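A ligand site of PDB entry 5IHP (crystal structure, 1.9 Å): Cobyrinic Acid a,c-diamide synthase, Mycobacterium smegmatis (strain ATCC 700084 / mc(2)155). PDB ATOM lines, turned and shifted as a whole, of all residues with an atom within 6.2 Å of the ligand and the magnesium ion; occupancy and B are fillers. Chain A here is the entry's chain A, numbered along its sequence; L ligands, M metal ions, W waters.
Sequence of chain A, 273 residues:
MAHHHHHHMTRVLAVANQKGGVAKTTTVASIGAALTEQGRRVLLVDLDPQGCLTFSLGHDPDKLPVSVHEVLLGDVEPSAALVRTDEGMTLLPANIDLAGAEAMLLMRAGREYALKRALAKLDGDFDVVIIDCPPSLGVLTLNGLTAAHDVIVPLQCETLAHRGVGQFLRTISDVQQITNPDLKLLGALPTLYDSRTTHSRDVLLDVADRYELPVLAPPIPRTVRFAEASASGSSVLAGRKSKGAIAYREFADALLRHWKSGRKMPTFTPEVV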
ATOM      1  N   ASN A  17       1.341  -7.516  24.800  1.00  0.00           N
ATOM      2  CA  ASN A  17       1.538  -6.436  25.759  1.00  0.00           C
ATOM      3  C   ASN A  17       2.432  -5.405  25.070  1.00  0.00           C
ATOM      4  O   ASN A  17       3.513  -5.758  24.586  1.00  0.00           O
ATOM      5  CB  ASN A  17       2.158  -6.940  27.073  1.00  0.00           C
ATOM      6  CG  ASN A  17       2.208  -5.862  28.154  1.00  0.00           C
ATOM      7  OD1 ASN A  17       2.165  -4.659  27.868  1.00  0.00           O
ATOM      8  ND2 ASN A  17       2.331  -6.294  29.419  1.00  0.00           N
ATOM      9  N   LYS A  19       4.062  -3.041  26.334  1.00  0.00           N
ATOM     10  CA  LYS A  19       5.226  -2.773  27.169  1.00  0.00           C
ATOM     11  C   LYS A  19       6.313  -3.801  26.884  1.00  0.00           C
ATOM     12  O   LYS A  19       6.029  -5.002  26.859  1.00  0.00           O
ATOM     13  CB  LYS A  19       4.833  -2.812  28.652  1.00  0.00           C
ATOM     14  CG  LYS A  19       5.880  -2.274  29.649  1.00  0.00           C
ATOM     15  CD  LYS A  19       6.195  -0.801  29.387  1.00  0.00           C
ATOM     16  CE  LYS A  19       7.173  -0.265  30.406  1.00  0.00           C
ATOM     17  NZ  LYS A  19       6.632  -0.462  31.779  1.00  0.00           N
ATOM     18  N   GLY A  20       7.544  -3.355  26.656  1.00  0.00           N
ATOM     19  CA  GLY A  20       8.637  -4.270  26.418  1.00  0.00           C
ATOM     20  C   GLY A  20       9.281  -4.759  27.702  1.00  0.00           C
ATOM     21  O   GLY A  20       9.236  -4.099  28.726  1.00  0.00           O
ATOM     22  N   GLY A  21       9.897  -5.945  27.634  1.00  0.00           N
ATOM     23  CA  GLY A  21      10.656  -6.442  28.759  1.00  0.00           C
ATOM     24  C   GLY A  21       9.818  -7.098  29.834  1.00  0.00           C
ATOM     25  O   GLY A  21      10.213  -7.114  30.997  1.00  0.00           O
ATOM     26  N   VAL A  22       8.649  -7.627  29.487  1.00  0.00           N
ATOM     27  CA  VAL A  22       7.729  -8.218  30.450  1.00  0.00           C
ATOM     28  C   VAL A  22       7.671  -9.728  30.311  1.00  0.00           C
ATOM     29  O   VAL A  22       6.759 -10.373  30.844  1.00  0.00           O
ATOM     30  CB  VAL A  22       6.320  -7.610  30.350  1.00  0.00           C
ATOM     31  CG1 VAL A  22       6.356  -6.120  30.663  1.00  0.00           C
ATOM     32  CG2 VAL A  22       5.705  -7.887  28.971  1.00  0.00           C
ATOM     33  N   ALA A  23       8.626 -10.303  29.571  1.00  0.00           N
ATOM     34  CA  ALA A  23       8.779 -11.755  29.363  1.00  0.00           C
ATOM     35  C   ALA A  23       7.723 -12.326  28.404  1.00  0.00           C
ATOM     36  O   ALA A  23       7.359 -13.491  28.534  1.00  0.00           O
ATOM     37  CB  ALA A  23       8.785 -12.527  30.689  1.00  0.00           C
ATOM     38  N   LYS A  24       7.244 -11.544  27.434  1.00  0.00           N
ATOM     39  CA  LYS A  24       6.360 -12.108  26.416  1.00  0.00           C
ATOM     40  C   LYS A  24       7.060 -13.233  25.660  1.00  0.00           C
ATOM     41  O   LYS A  24       6.526 -14.345  25.558  1.00  0.00           O
ATOM     42  CB  LYS A  24       5.899 -11.043  25.426  1.00  0.00           C
ATOM     43  CG  LYS A  24       5.097  -9.935  26.043  1.00  0.00           C
ATOM     44  CD  LYS A  24       3.893  -9.620  25.240  1.00  0.00           C
ATOM     45  CE  LYS A  24       4.298  -9.310  23.829  1.00  0.00           C
ATOM     46  NZ  LYS A  24       5.048  -8.046  23.757  1.00  0.00           N
ATOM     47  N   THR A  25       8.237 -12.953  25.110  1.00  0.00           N
ATOM     48  CA  THR A  25       8.909 -13.920  24.248  1.00  0.00           C
ATOM     49  C   THR A  25       9.308 -15.172  25.027  1.00  0.00           C
ATOM     50  O   THR A  25       9.101 -16.298  24.555  1.00  0.00           O
ATOM     51  CB  THR A  25      10.133 -13.256  23.591  1.00  0.00           C
ATOM     52  OG1 THR A  25       9.677 -12.258  22.674  1.00  0.00           O
ATOM     53  CG2 THR A  25      11.011 -14.283  22.858  1.00  0.00           C
ATOM     54  N   THR A  26       9.868 -14.991  26.220  1.00  0.00           N
ATOM     55  CA  THR A  26      10.161 -16.118  27.092  1.00  0.00           C
ATOM     56  C   THR A  26       8.906 -16.939  27.359  1.00  0.00           C
ATOM     57  O   THR A  26       8.954 -18.178  27.397  1.00  0.00           O
ATOM     58  CB  THR A  26      10.763 -15.627  28.409  1.00  0.00           C
ATOM     59  OG1 THR A  26      11.958 -14.865  28.161  1.00  0.00           O
ATOM     60  CG2 THR A  26      11.099 -16.793  29.337  1.00  0.00           C
ATOM     61  N   THR A  27       7.772 -16.253  27.545  1.00  0.00           N
ATOM     62  CA  THR A  27       6.508 -16.928  27.824  1.00  0.00           C
ATOM     63  C   THR A  27       6.051 -17.746  26.636  1.00  0.00           C
ATOM     64  O   THR A  27       5.623 -18.904  26.796  1.00  0.00           O
ATOM     65  CB  THR A  27       5.436 -15.898  28.229  1.00  0.00           C
ATOM     66  OG1 THR A  27       5.734 -15.361  29.533  1.00  0.00           O
ATOM     67  CG2 THR A  27       4.053 -16.517  28.243  1.00  0.00           C
ATOM     68  N   ASP A  48       7.706 -10.171  15.941  1.00  0.00           N
ATOM     69  CA  ASP A  48       8.567  -9.036  16.276  1.00  0.00           C
ATOM     70  C   ASP A  48       9.669  -8.934  15.231  1.00  0.00           C
ATOM     71  O   ASP A  48      10.468  -9.877  15.091  1.00  0.00           O
ATOM     72  CB  ASP A  48       9.177  -9.232  17.661  1.00  0.00           C
ATOM     73  CG  ASP A  48       9.814  -7.948  18.191  1.00  0.00           C
ATOM     74  OD1 ASP A  48      10.148  -7.066  17.384  1.00  0.00           O
ATOM     75  OD2 ASP A  48       9.992  -7.845  19.423  1.00  0.00           O
ATOM     76  N   CYS A  52      13.397 -11.698  18.406  1.00  0.00           N
ATOM     77  CA  CYS A  52      13.890 -12.244  19.676  1.00  0.00           C
ATOM     78  C   CYS A  52      13.548 -13.716  19.825  1.00  0.00           C
ATOM     79  O   CYS A  52      14.393 -14.523  20.228  1.00  0.00           O
ATOM     80  CB  CYS A  52      13.327 -11.458  20.847  1.00  0.00           C
ATOM     81  SG  CYS A  52      13.578  -9.687  20.665  1.00  0.00           S
ATOM     82  N   LEU A  53      12.295 -14.088  19.526  1.00  0.00           N
ATOM     83  CA  LEU A  53      11.890 -15.483  19.647  1.00  0.00           C
ATOM     84  C   LEU A  53      12.681 -16.362  18.701  1.00  0.00           C
ATOM     85  O   LEU A  53      13.186 -17.426  19.078  1.00  0.00           O
ATOM     86  CB  LEU A  53      10.388 -15.626  19.350  1.00  0.00           C
ATOM     87  CG  LEU A  53       9.868 -17.065  19.379  1.00  0.00           C
ATOM     88  CD1 LEU A  53       9.962 -17.617  20.801  1.00  0.00           C
ATOM     89  CD2 LEU A  53       8.452 -17.135  18.837  1.00  0.00           C
ATOM     90  N   ASP A 132       3.810 -14.524  19.289  1.00  0.00           N
ATOM     91  CA  ASP A 132       4.600 -13.590  20.084  1.00  0.00           C
ATOM     92  C   ASP A 132       4.458 -12.210  19.454  1.00  0.00           C
ATOM     93  O   ASP A 132       5.034 -11.941  18.392  1.00  0.00           O
ATOM     94  CB  ASP A 132       6.050 -14.048  20.119  1.00  0.00           C
ATOM     95  CG  ASP A 132       6.921 -13.195  21.053  1.00  0.00           C
ATOM     96  OD1 ASP A 132       6.374 -12.477  21.924  1.00  0.00           O
ATOM     97  OD2 ASP A 132       8.161 -13.286  20.908  1.00  0.00           O
ATOM     98  N   CYS A 133       3.677 -11.297  20.123  1.00  0.00           N
ATOM     99  CA  CYS A 133       3.463  -9.987  19.531  1.00  0.00           C
ATOM    100  C   CYS A 133       4.581  -9.021  19.931  1.00  0.00           C
ATOM    101  O   CYS A 133       5.190  -9.186  20.992  1.00  0.00           O
ATOM    102  CB  CYS A 133       2.112  -9.419  19.988  1.00  0.00           C
ATOM    103  SG  CYS A 133       0.680 -10.375  19.389  1.00  0.00           S
ATOM    104  N   PRO A 134       4.903  -8.060  19.064  1.00  0.00           N
ATOM    105  CA  PRO A 134       5.921  -7.066  19.389  1.00  0.00           C
ATOM    106  C   PRO A 134       5.412  -6.117  20.463  1.00  0.00           C
ATOM    107  O   PRO A 134       4.205  -6.094  20.754  1.00  0.00           O
ATOM    108  CB  PRO A 134       6.122  -6.328  18.058  1.00  0.00           C
ATOM    109  CG  PRO A 134       4.772  -6.417  17.397  1.00  0.00           C
ATOM    110  CD  PRO A 134       4.292  -7.806  17.743  1.00  0.00           C
ATOM    111  N   PRO A 135       6.324  -5.317  21.110  1.00  0.00           N
ATOM    112  CA  PRO A 135       5.902  -4.330  22.126  1.00  0.00           C
ATOM    113  C   PRO A 135       5.361  -3.076  21.441  1.00  0.00           C
ATOM    114  O   PRO A 135       6.012  -2.017  21.395  1.00  0.00           O
ATOM    115  CB  PRO A 135       7.197  -4.053  22.894  1.00  0.00           C
ATOM    116  CG  PRO A 135       8.298  -4.256  21.827  1.00  0.00           C
ATOM    117  CD  PRO A 135       7.807  -5.416  20.998  1.00  0.00           C
ATOM    118  N   PRO A 154       1.232 -11.163  29.424  1.00  0.00           N
ATOM    119  CA  PRO A 154       2.301 -11.268  30.416  1.00  0.00           C
ATOM    120  C   PRO A 154       2.475  -9.904  31.064  1.00  0.00           C
ATOM    121  O   PRO A 154       2.575  -8.888  30.375  1.00  0.00           O
ATOM    122  CB  PRO A 154       3.529 -11.666  29.594  1.00  0.00           C
ATOM    123  CG  PRO A 154       2.965 -12.311  28.386  1.00  0.00           C
ATOM    124  CD  PRO A 154       1.712 -11.510  28.075  1.00  0.00           C
ATOM    125  N   LEU A 192       8.054 -12.051  36.316  1.00  0.00           N
ATOM    126  CA  LEU A 192       9.104 -11.417  37.120  1.00  0.00           C
ATOM    127  C   LEU A 192       8.656 -11.272  38.572  1.00  0.00           C
ATOM    128  O   LEU A 192       8.994 -10.294  39.252  1.00  0.00           O
ATOM    129  CB  LEU A 192       9.522 -10.065  36.533  1.00  0.00           C
ATOM    130  CG  LEU A 192       9.957 -10.095  35.061  1.00  0.00           C
ATOM    131  CD1 LEU A 192      10.332  -8.693  34.593  1.00  0.00           C
ATOM    132  CD2 LEU A 192      11.100 -11.054  34.857  1.00  0.00           C
ATOM    133  N   ILE A 220       4.846 -16.407  37.339  1.00  0.00           N
ATOM    134  CA  ILE A 220       6.156 -16.870  36.911  1.00  0.00           C
ATOM    135  C   ILE A 220       7.198 -16.128  37.731  1.00  0.00           C
ATOM    136  O   ILE A 220       7.270 -14.891  37.645  1.00  0.00           O
ATOM    137  CB  ILE A 220       6.398 -16.659  35.415  1.00  0.00           C
ATOM    138  CG1 ILE A 220       5.181 -17.094  34.582  1.00  0.00           C
ATOM    139  CG2 ILE A 220       7.669 -17.397  34.991  1.00  0.00           C
ATOM    140  CD1 ILE A 220       4.786 -18.570  34.778  1.00  0.00           C
ATOM    141  N   PRO A 221       8.020 -16.812  38.525  1.00  0.00           N
ATOM    142  CA  PRO A 221       9.008 -16.102  39.346  1.00  0.00           C
ATOM    143  C   PRO A 221      10.152 -15.558  38.510  1.00  0.00           C
ATOM    144  O   PRO A 221      10.473 -16.070  37.432  1.00  0.00           O
ATOM    145  CB  PRO A 221       9.502 -17.185  40.313  1.00  0.00           C
ATOM    146  CG  PRO A 221       9.296 -18.475  39.557  1.00  0.00           C
ATOM    147  CD  PRO A 221       8.031 -18.270  38.760  1.00  0.00           C
ATOM    148  N   ARG A 222      10.782 -14.491  39.011  1.00  0.00           N
ATOM    149  CA  ARG A 222      12.047 -14.047  38.450  1.00  0.00           C
ATOM    150  C   ARG A 222      13.120 -15.088  38.761  1.00  0.00           C
ATOM    151  O   ARG A 222      13.245 -15.539  39.901  1.00  0.00           O
ATOM    152  CB  ARG A 222      12.461 -12.689  39.000  1.00  0.00           C
ATOM    153  CG  ARG A 222      13.892 -12.313  38.610  1.00  0.00           C
ATOM    154  CD  ARG A 222      14.415 -11.056  39.303  1.00  0.00           C
ATOM    155  NE  ARG A 222      13.838  -9.826  38.761  1.00  0.00           N
ATOM    156  CZ  ARG A 222      14.153  -9.299  37.570  1.00  0.00           C
ATOM    157  NH1 ARG A 222      15.040  -9.896  36.785  1.00  0.00           N
ATOM    158  NH2 ARG A 222      13.569  -8.179  37.175  1.00  0.00           N
ATOM    159  N   THR A 223      13.890 -15.465  37.742  1.00  0.00           N
ATOM    160  CA  THR A 223      14.827 -16.583  37.823  1.00  0.00           C
ATOM    161  C   THR A 223      16.262 -16.101  37.965  1.00  0.00           C
ATOM    162  O   THR A 223      16.504 -14.961  38.359  1.00  0.00           O
ATOM    163  CB  THR A 223      14.724 -17.489  36.580  1.00  0.00           C
ATOM    164  N   GLY A 244      10.828 -21.380  37.713  1.00  0.00           N
ATOM    165  CA  GLY A 244      10.200 -20.770  36.560  1.00  0.00           C
ATOM    166  C   GLY A 244       9.632 -21.796  35.590  1.00  0.00           C
ATOM    167  O   GLY A 244       8.518 -21.638  35.094  1.00  0.00           O
ATOM    168  N   TYR A 248       5.682 -22.412  34.522  1.00  0.00           N
ATOM    169  CA  TYR A 248       5.221 -22.435  33.132  1.00  0.00           C
ATOM    170  C   TYR A 248       4.503 -23.745  32.808  1.00  0.00           C
ATOM    171  O   TYR A 248       3.485 -23.736  32.107  1.00  0.00           O
ATOM    172  CB  TYR A 248       6.400 -22.219  32.200  1.00  0.00           C
ATOM    173  CG  TYR A 248       6.712 -20.754  31.914  1.00  0.00           C
ATOM    174  CD1 TYR A 248       5.728 -19.880  31.453  1.00  0.00           C
ATOM    175  CD2 TYR A 248       7.991 -20.258  32.107  1.00  0.00           C
ATOM    176  CE1 TYR A 248       6.011 -18.537  31.187  1.00  0.00           C
ATOM    177  CE2 TYR A 248       8.290 -18.924  31.828  1.00  0.00           C
ATOM    178  CZ  TYR A 248       7.301 -18.076  31.386  1.00  0.00           C
ATOM    179  OH  TYR A 248       7.622 -16.758  31.132  1.00  0.00           O
HETATM  180  P1  LIG L   1       9.520  -9.250  26.083  1.00  0.00           P
HETATM  181  O1  LIG L   1       8.240  -8.919  26.807  1.00  0.00           O
HETATM  182  O2  LIG L   1      10.329  -8.046  25.654  1.00  0.00           O
HETATM  183  O3  LIG L   1       9.374 -10.286  24.986  1.00  0.00           O
HETATM  184  P2  LIG L   1      11.535 -11.130  26.987  1.00  0.00           P
HETATM  185  O4  LIG L   1      10.961 -12.529  27.053  1.00  0.00           O
HETATM  186  O5  LIG L   1      12.471 -10.731  25.857  1.00  0.00           O
HETATM  187  O6  LIG L   1      10.390 -10.023  27.218  1.00  0.00           O
HETATM  188  O7  LIG L   1      12.332 -10.919  28.374  1.00  0.00           O
HETATM  189  C1  LIG L   1      12.966  -9.666  28.633  1.00  0.00           C
HETATM  190  C2  LIG L   1      14.186  -9.940  29.494  1.00  0.00           C
HETATM  191  O8  LIG L   1      13.769 -10.539  30.723  1.00  0.00           O
HETATM  192  C3  LIG L   1      15.113 -10.937  28.832  1.00  0.00           C
HETATM  193  O9  LIG L   1      16.457 -10.526  29.101  1.00  0.00           O
HETATM  194  C4  LIG L   1      14.868 -12.249  29.543  1.00  0.00           C
HETATM  195  O10 LIG L   1      16.059 -13.034  29.583  1.00  0.00           O
HETATM  196  C5  LIG L   1      14.459 -11.775  30.918  1.00  0.00           C
HETATM  197  N1  LIG L   1      13.549 -12.721  31.597  1.00  0.00           N
HETATM  198  C6  LIG L   1      12.428 -13.274  31.083  1.00  0.00           C
HETATM  199  N2  LIG L   1      11.845 -14.094  31.990  1.00  0.00           N
HETATM  200  C7  LIG L   1      12.595 -14.071  33.104  1.00  0.00           C
HETATM  201  C8  LIG L   1      12.539 -14.700  34.446  1.00  0.00           C
HETATM  202  N3  LIG L   1      11.529 -15.551  34.766  1.00  0.00           N
HETATM  203  N4  LIG L   1      13.519 -14.399  35.328  1.00  0.00           N
HETATM  204  C9  LIG L   1      14.516 -13.552  35.020  1.00  0.00           C
HETATM  205  N5  LIG L   1      14.626 -12.953  33.816  1.00  0.00           N
HETATM  206  C10 LIG L   1      13.714 -13.168  32.840  1.00  0.00           C
HETATM  207 MG    MG M   1       9.694 -10.117  22.973  1.00  0.00          MG
HETATM  208  O   HOH W   1       7.493 -10.221  22.424  1.00  0.00           O
HETATM  209  O   HOH W   2       9.604 -15.514  32.671  1.00  0.00           O
HETATM  210  O   HOH W   3       9.181 -14.160  35.082  1.00  0.00           O
HETATM  211  O   HOH W   4      11.387  -6.259  23.347  1.00  0.00           O
HETATM  212  O   HOH W   5      12.675  -7.155  25.423  1.00  0.00           O
HETATM  213  O   HOH W   6      10.189  -9.974  20.804  1.00  0.00           O
HETATM  214  O   HOH W   7       9.533  -8.006  23.009  1.00  0.00           O
HETATM  215  O   HOH W   8      14.972  -9.428  25.340  1.00  0.00           O
HETATM  216  O   HOH W   9       6.772  -7.273  25.367  1.00  0.00           O
HETATM  217  O   HOH W  10      11.813 -10.094  23.295  1.00  0.00           O
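The side-chain hydroxyl of Thr 25 sits close to the side-chain carboxylate of Asp 132 (2.5 Å).
NZ of Lys 24 sits close to O of Cys 133 (3.0 Å).
The side-chain amino group (NZ) of Lys 24 is in hydrogen-bond range of the backbone carbonyl oxygen (O) of Asn 17 (2.9 Å).
OG1 of Thr 27 sits at hydrogen-bond distance from O of Ala 23.
The backbone NH (N) of Leu 192 sits at hydrogen-bond distance from the backbone carbonyl oxygen (O) of Ile 220 (3.2 Å).
Of the 25 residues printed, 1 comes within 4 Å of the magnesium ion.
The magnesium ion is bound by O3 of the ligand (2.0 Å), water W7 (2.1 Å), water W10 (2.1 Å), OG1 of Thr 25 (2.2 Å), water W6 (2.2 Å) and water W1 (2.3 Å).
The magnesium ion has six donor atoms within binding distance.
CD2 of Leu 192 touches C7 of the ligand (3.8 Å).
Arg 222 touches the ligand (CA to N4, 3.5 Å).
Hydrophobic or aromatic side chains that line the ligand: Val 22, Ala 23 and Leu 192.
The nearest printed residue that does not touch the ligand is Gly 20 (4.01 Å).
The backbone NH of Thr 25 sits at hydrogen-bond distance from an oxygen (O4) of the ligand.
N of Thr 223 sits at hydrogen-bond distance from N4 of the ligand (2.7 Å).
An oxygen (O4) of the ligand sits at hydrogen-bond distance from the backbone NH (N) of Thr 26 (2.8 Å).
An oxygen (O4) of the ligand sits at hydrogen-bond distance from the side-chain hydroxyl (OG1) of Thr 26 (2.8 Å).
O1 of the ligand is in hydrogen-bond range of N of Lys 24, at 2.9 Å.
The backbone carbonyl oxygen (O) of Pro 221 is in hydrogen-bond range of a nitrogen (N3) of the ligand, at 2.9 Å.
The backbone NH (N) of Gly 21 sits at hydrogen-bond distance from an oxygen (O2) of the ligand, at 2.9 Å.
N of Ala 23 sits at hydrogen-bond distance from O6 of the ligand (3.0 Å).
O1 of the ligand sits at hydrogen-bond distance from N of Val 22.
Water W1 bridges OD1 of Asp 132 (2.6 Å) and O of Cys 133 (2.9 Å).
Water W6 lies within hydrogen-bond range of OD2 of Asp 48 (2.5 Å) and SG of Cys 52 (3.4 Å).
Water W10 lies within hydrogen-bond range of O5 of the ligand (2.7 Å) and SG of Cys 52 (3.2 Å).
Water W9 lies within hydrogen-bond range of NZ of Lys 24 (2.5 Å), O1 of the ligand (2.6 Å) and O of Lys 19 (2.8 Å).
Water W2 lies within hydrogen-bond range of a nitrogen (N2) of the ligand (2.7 Å) and the side-chain hydroxyl of Tyr 248 (2.8 Å).
Water W3 lies within hydrogen-bond range of N of Leu 192 (2.7 Å), N3 of the ligand (2.7 Å), O of Ile 220 (3.3 Å) and O of Pro 221 (3.3 Å).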
